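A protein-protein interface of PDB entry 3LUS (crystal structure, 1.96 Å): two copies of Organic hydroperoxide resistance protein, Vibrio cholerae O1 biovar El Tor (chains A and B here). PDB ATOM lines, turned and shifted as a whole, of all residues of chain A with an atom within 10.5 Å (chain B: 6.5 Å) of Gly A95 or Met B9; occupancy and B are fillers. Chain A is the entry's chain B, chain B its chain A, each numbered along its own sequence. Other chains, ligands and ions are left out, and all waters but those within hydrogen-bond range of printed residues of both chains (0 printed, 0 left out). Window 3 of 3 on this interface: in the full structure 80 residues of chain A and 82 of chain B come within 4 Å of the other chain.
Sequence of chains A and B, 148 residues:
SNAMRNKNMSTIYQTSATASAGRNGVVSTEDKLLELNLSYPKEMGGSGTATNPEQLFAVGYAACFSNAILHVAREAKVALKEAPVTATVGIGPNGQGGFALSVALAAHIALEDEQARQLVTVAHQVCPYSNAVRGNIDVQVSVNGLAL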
ATOM      1  N   GLY A  90     -11.915 -17.532 -17.221  1.00  0.00           N
ATOM      2  CA  GLY A  90     -12.583 -18.088 -18.408  1.00  0.00           C
ATOM      3  C   GLY A  90     -14.103 -17.957 -18.322  1.00  0.00           C
ATOM      4  O   GLY A  90     -14.695 -17.843 -17.217  1.00  0.00           O
ATOM      5  N   ILE A  91     -14.741 -17.944 -19.486  1.00  0.00           N
ATOM      6  CA  ILE A  91     -16.206 -17.895 -19.529  1.00  0.00           C
ATOM      7  C   ILE A  91     -16.623 -18.985 -20.490  1.00  0.00           C
ATOM      8  O   ILE A  91     -15.982 -19.225 -21.519  1.00  0.00           O
ATOM      9  CB  ILE A  91     -16.784 -16.533 -19.981  1.00  0.00           C
ATOM     10  CG1 ILE A  91     -18.308 -16.631 -20.068  1.00  0.00           C
ATOM     11  CG2 ILE A  91     -16.195 -16.079 -21.298  1.00  0.00           C
ATOM     12  CD1 ILE A  91     -19.004 -15.310 -20.175  1.00  0.00           C
ATOM     13  N   GLY A  92     -17.680 -19.680 -20.139  1.00  0.00           N
ATOM     14  CA  GLY A  92     -18.193 -20.706 -21.020  1.00  0.00           C
ATOM     15  C   GLY A  92     -19.610 -21.027 -20.574  1.00  0.00           C
ATOM     16  O   GLY A  92     -20.106 -20.487 -19.570  1.00  0.00           O
ATOM     17  N   PRO A  93     -20.313 -21.848 -21.337  1.00  0.00           N
ATOM     18  CA  PRO A  93     -21.708 -22.168 -21.029  1.00  0.00           C
ATOM     19  C   PRO A  93     -21.846 -23.007 -19.795  1.00  0.00           C
ATOM     20  O   PRO A  93     -20.987 -23.763 -19.544  1.00  0.00           O
ATOM     21  CB  PRO A  93     -22.149 -22.993 -22.226  1.00  0.00           C
ATOM     22  CG  PRO A  93     -20.924 -23.510 -22.788  1.00  0.00           C
ATOM     23  CD  PRO A  93     -19.904 -22.456 -22.598  1.00  0.00           C
ATOM     24  N   ASN A  94     -22.942 -22.887 -19.069  1.00  0.00           N
ATOM     25  CA  ASN A  94     -23.160 -23.710 -17.897  1.00  0.00           C
ATOM     26  C   ASN A  94     -24.055 -24.917 -18.031  1.00  0.00           C
ATOM     27  O   ASN A  94     -24.245 -25.607 -17.092  1.00  0.00           O
ATOM     28  CB  ASN A  94     -23.633 -22.906 -16.690  1.00  0.00           C
ATOM     29  CG  ASN A  94     -24.936 -22.234 -16.904  1.00  0.00           C
ATOM     30  OD1 ASN A  94     -25.647 -22.511 -17.830  1.00  0.00           O
ATOM     31  ND2 ASN A  94     -25.258 -21.351 -16.027  1.00  0.00           N
ATOM     32  N   GLY A  95     -24.610 -25.212 -19.170  1.00  0.00           N
ATOM     33  CA  GLY A  95     -25.441 -26.405 -19.127  1.00  0.00           C
ATOM     34  C   GLY A  95     -26.861 -26.208 -18.662  1.00  0.00           C
ATOM     35  O   GLY A  95     -27.632 -27.108 -18.711  1.00  0.00           O
ATOM     36  N   GLN A  96     -27.188 -25.018 -18.205  1.00  0.00           N
ATOM     37  CA  GLN A  96     -28.553 -24.655 -17.880  1.00  0.00           C
ATOM     38  C   GLN A  96     -29.109 -23.530 -18.747  1.00  0.00           C
ATOM     39  O   GLN A  96     -30.192 -23.084 -18.520  1.00  0.00           O
ATOM     40  CB  GLN A  96     -28.703 -24.326 -16.392  1.00  0.00           C
ATOM     41  CG  GLN A  96     -27.779 -25.133 -15.521  1.00  0.00           C
ATOM     42  CD  GLN A  96     -28.384 -25.562 -14.227  1.00  0.00           C
ATOM     43  OE1 GLN A  96     -29.343 -24.959 -13.750  1.00  0.00           O
ATOM     44  NE2 GLN A  96     -27.826 -26.633 -13.634  1.00  0.00           N
ATOM     45  N   GLY A  97     -28.372 -23.107 -19.753  1.00  0.00           N
ATOM     46  CA  GLY A  97     -28.810 -22.026 -20.641  1.00  0.00           C
ATOM     47  C   GLY A  97     -28.144 -20.698 -20.386  1.00  0.00           C
ATOM     48  O   GLY A  97     -28.446 -19.723 -21.083  1.00  0.00           O
ATOM     49  N   GLY A  98     -27.276 -20.634 -19.363  1.00  0.00           N
ATOM     50  CA  GLY A  98     -26.545 -19.407 -19.025  1.00  0.00           C
ATOM     51  C   GLY A  98     -25.061 -19.622 -19.170  1.00  0.00           C
ATOM     52  O   GLY A  98     -24.605 -20.597 -19.784  1.00  0.00           O
ATOM     53  N   PHE A  99     -24.308 -18.713 -18.582  1.00  0.00           N
ATOM     54  CA  PHE A  99     -22.848 -18.703 -18.657  1.00  0.00           C
ATOM     55  C   PHE A  99     -22.283 -18.637 -17.251  1.00  0.00           C
ATOM     56  O   PHE A  99     -22.946 -18.079 -16.316  1.00  0.00           O
ATOM     57  CB  PHE A  99     -22.351 -17.504 -19.487  1.00  0.00           C
ATOM     58  CG  PHE A  99     -22.861 -17.570 -20.913  1.00  0.00           C
ATOM     59  CD1 PHE A  99     -22.158 -18.267 -21.880  1.00  0.00           C
ATOM     60  CD2 PHE A  99     -24.085 -17.011 -21.254  1.00  0.00           C
ATOM     61  CE1 PHE A  99     -22.648 -18.383 -23.176  1.00  0.00           C
ATOM     62  CE2 PHE A  99     -24.582 -17.145 -22.565  1.00  0.00           C
ATOM     63  CZ  PHE A  99     -23.847 -17.828 -23.519  1.00  0.00           C
ATOM     64  N   ALA A 100     -21.061 -19.153 -17.132  1.00  0.00           N
ATOM     65  CA  ALA A 100     -20.359 -19.216 -15.854  1.00  0.00           C
ATOM     66  C   ALA A 100     -18.901 -18.821 -16.037  1.00  0.00           C
ATOM     67  O   ALA A 100     -18.341 -18.994 -17.093  1.00  0.00           O
ATOM     68  CB  ALA A 100     -20.439 -20.600 -15.247  1.00  0.00           C
ATOM     69  N   LEU A 101     -18.308 -18.265 -14.986  1.00  0.00           N
ATOM     70  CA  LEU A 101     -16.906 -17.948 -15.009  1.00  0.00           C
ATOM     71  C   LEU A 101     -16.155 -19.081 -14.341  1.00  0.00           C
ATOM     72  O   LEU A 101     -16.625 -19.708 -13.398  1.00  0.00           O
ATOM     73  CB  LEU A 101     -16.648 -16.655 -14.220  1.00  0.00           C
ATOM     74  CG  LEU A 101     -17.300 -15.374 -14.758  1.00  0.00           C
ATOM     75  CD1 LEU A 101     -17.033 -14.161 -13.831  1.00  0.00           C
ATOM     76  CD2 LEU A 101     -16.972 -15.103 -16.256  1.00  0.00           C
ATOM     77  N   SER A 102     -14.950 -19.281 -14.777  1.00  0.00           N
ATOM     78  CA  SER A 102     -13.976 -20.141 -14.091  1.00  0.00           C
ATOM     79  C   SER A 102     -12.797 -19.195 -13.738  1.00  0.00           C
ATOM     80  O   SER A 102     -12.554 -18.202 -14.456  1.00  0.00           O
ATOM     81  CB  SER A 102     -13.556 -21.334 -15.032  1.00  0.00           C
ATOM     82  OG  SER A 102     -12.912 -20.801 -16.207  1.00  0.00           O
ATOM     83  N   ASN A 136     -19.750 -20.792  -5.542  1.00  0.00           N
ATOM     84  CA  ASN A 136     -20.209 -20.703  -6.910  1.00  0.00           C
ATOM     85  C   ASN A 136     -19.086 -20.979  -7.888  1.00  0.00           C
ATOM     86  O   ASN A 136     -19.203 -21.793  -8.786  1.00  0.00           O
ATOM     87  CB  ASN A 136     -20.832 -19.348  -7.207  1.00  0.00           C
ATOM     88  CG  ASN A 136     -22.098 -19.091  -6.410  1.00  0.00           C
ATOM     89  OD1 ASN A 136     -22.383 -17.962  -5.972  1.00  0.00           O
ATOM     90  ND2 ASN A 136     -22.872 -20.122  -6.244  1.00  0.00           N
ATOM     91  N   ARG B   5     -25.346 -24.862 -12.875  1.00  0.00           N
ATOM     92  CA  ARG B   5     -25.478 -23.362 -12.937  1.00  0.00           C
ATOM     93  C   ARG B   5     -24.112 -22.711 -12.936  1.00  0.00           C
ATOM     94  O   ARG B   5     -23.878 -21.641 -13.559  1.00  0.00           O
ATOM     95  CB  ARG B   5     -26.271 -22.811 -11.741  1.00  0.00           C
ATOM     96  N   LYS B   7     -20.982 -24.371 -13.425  1.00  0.00           N
ATOM     97  CA  LYS B   7     -19.836 -24.967 -14.089  1.00  0.00           C
ATOM     98  C   LYS B   7     -19.710 -24.306 -15.459  1.00  0.00           C
ATOM     99  O   LYS B   7     -20.664 -24.308 -16.244  1.00  0.00           O
ATOM    100  CB  LYS B   7     -20.036 -26.488 -14.209  1.00  0.00           C
ATOM    101  CG  LYS B   7     -18.769 -27.238 -14.640  1.00  0.00           C
ATOM    102  CD  LYS B   7     -18.857 -28.753 -14.415  1.00  0.00           C
ATOM    103  CE  LYS B   7     -17.442 -29.320 -14.132  1.00  0.00           C
ATOM    104  NZ  LYS B   7     -17.451 -30.825 -13.963  1.00  0.00           N
ATOM    105  N   ASN B   8     -18.541 -23.776 -15.743  1.00  0.00           N
ATOM    106  CA  ASN B   8     -18.157 -23.403 -17.065  1.00  0.00           C
ATOM    107  C   ASN B   8     -17.736 -24.678 -17.762  1.00  0.00           C
ATOM    108  O   ASN B   8     -16.666 -25.179 -17.526  1.00  0.00           O
ATOM    109  CB  ASN B   8     -17.014 -22.415 -17.013  1.00  0.00           C
ATOM    110  CG  ASN B   8     -16.201 -22.387 -18.252  1.00  0.00           C
ATOM    111  OD1 ASN B   8     -16.615 -22.821 -19.288  1.00  0.00           O
ATOM    112  ND2 ASN B   8     -15.012 -21.865 -18.141  1.00  0.00           N
ATOM    113  N   MET B   9     -18.594 -25.183 -18.631  1.00  0.00           N
ATOM    114  CA  MET B   9     -18.429 -26.473 -19.260  1.00  0.00           C
ATOM    115  C   MET B   9     -17.482 -26.554 -20.424  1.00  0.00           C
ATOM    116  O   MET B   9     -17.044 -27.599 -20.775  1.00  0.00           O
ATOM    117  CB  MET B   9     -19.774 -27.001 -19.675  1.00  0.00           C
ATOM    118  CG  MET B   9     -20.526 -27.412 -18.495  1.00  0.00           C
ATOM    119  SD  MET B   9     -22.120 -28.230 -18.961  1.00  0.00           S
ATOM    120  CE  MET B   9     -21.432 -29.988 -19.210  1.00  0.00           C
ATOM    121  N   SER B  10     -17.164 -25.428 -20.998  1.00  0.00           N
ATOM    122  CA  SER B  10     -16.254 -25.393 -22.071  1.00  0.00           C
ATOM    123  C   SER B  10     -15.904 -23.950 -22.329  1.00  0.00           C
ATOM    124  O   SER B  10     -16.733 -23.187 -22.657  1.00  0.00           O
ATOM    125  CB  SER B  10     -16.875 -25.996 -23.295  1.00  0.00           C
ATOM    126  OG  SER B  10     -16.095 -25.737 -24.396  1.00  0.00           O
ATOM    127  N   THR B  11     -14.648 -23.616 -22.196  1.00  0.00           N
ATOM    128  CA  THR B  11     -14.244 -22.232 -22.140  1.00  0.00           C
ATOM    129  C   THR B  11     -14.284 -21.688 -23.523  1.00  0.00           C
ATOM    130  O   THR B  11     -13.618 -22.177 -24.382  1.00  0.00           O
ATOM    131  CB  THR B  11     -12.824 -22.134 -21.567  1.00  0.00           C
ATOM    132  OG1 THR B  11     -12.901 -22.611 -20.233  1.00  0.00           O
ATOM    133  CG2 THR B  11     -12.308 -20.685 -21.565  1.00  0.00           C
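The backbone NH (N) of Arg B5 sits close to the side-chain amide nitrogen (NE2) of Gln A96.
The side-chain amide nitrogen (ND2) of Asn B8 sits at hydrogen-bond distance from the side-chain hydroxyl (OG) of Ser A102.
The backbone NH (N) of Met B9 sits at hydrogen-bond distance from the backbone carbonyl oxygen (O) of Pro A93 (2.9 Å).
The backbone carbonyl oxygen (O) of Lys B7 lies close to the backbone carbonyl oxygen (O) of Pro A93 (3.4 Å).
OD1 of Asn B8 lies close to N of Gly A92, 3.4 Å away.
The side-chain amide nitrogen of Asn A94 lies within hydrogen-bond range of the backbone carbonyl oxygen of Arg B5.
OD1 of Asn A94 lies within hydrogen-bond range of N of Gly A97, 3.4 Å away.
OD1 of Asn B8 sits at hydrogen-bond distance from N of Ser B10 (3.2 Å).
N of Gly A98 lies within hydrogen-bond range of OD1 of Asn A94 (2.9 Å).
The backbone NH of Ala A100 lies within hydrogen-bond range of the backbone carbonyl oxygen of Gly A92 (2.9 Å).
N of Gln A96 is in hydrogen-bond range of OD1 of Asn A94, at 3.0 Å.
The side-chain amide nitrogen of Asn B8 sits at hydrogen-bond distance from the side-chain hydroxyl of Thr B11, 3.1 Å away.
Among the printed residues, merely in contact across the chains: Ile A91 with Thr B11, Gly A92 with Ser B10, Pro A93 with Asn B8, Pro A93 with Ser B10, Asn A94 with Lys B7, Asn A94 with Met B9, Gly A95 with Met B9, Ala A100 with Arg B5, Ala A100 with Lys B7 and Ala A100 with Asn B8.
Gly A95 touches just one residue of chain B: Met B9 (3.8 Å).
Of chain A, only Pro A93 (2.9 Å), Asn A94 (3.9 Å) and Gly A95 (3.8 Å) come within 4 Å of Met B9.
Of chain A, only Gly A92 (3.3 Å) and Pro A93 (3.3 Å) come within 4 Å of Ser B10.
Printed residues of chain A within 4 Å of Lys B7: Pro A93 (3.4 Å), Asn A94 (3.1 Å) and Ala A100 (3.8 Å).
Of the printed residues of chain B, Gln A96 touches Arg B5.
Of the printed residues of chain B, Ile A91 touches Thr B11.
Printed residues of chain B within 4 Å of Asn A94: Arg B5 (2.8 Å), Lys B7 (3.1 Å) and Met B9 (3.9 Å).
Of the printed residues of chain A, Thr B11 touches Ile A91 (3.5 Å).
Gly A90 touches none of the printed residues of chain B.
The nearest residue of chain A that does not touch Met B9 is Gly A92 (4.7 Å).
Hydrophobic or aromatic side chains of chain B that line the printed part of chain A: Met B9.
Of the 14 printed residues of chain A, 8 touch a printed residue of chain B.
Printed residues of chain A that touch a printed residue of chain B: Ile A91, Gly A92, Pro A93, Asn A94, Gly A95, Gln A96, Ala A100 and Ser A102.
Hydrophobic or aromatic side chains of chain A within 4 Å of the printed part of chain B: Pro A93 and Ala A100.
Among the printed residues, 16 pairs touch across the chains.
Among the printed residues, no Asp or Glu carboxylate lies within 4 Å of a Lys or Arg side-chain nitrogen of the other chain.
No position is printed for both chains.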
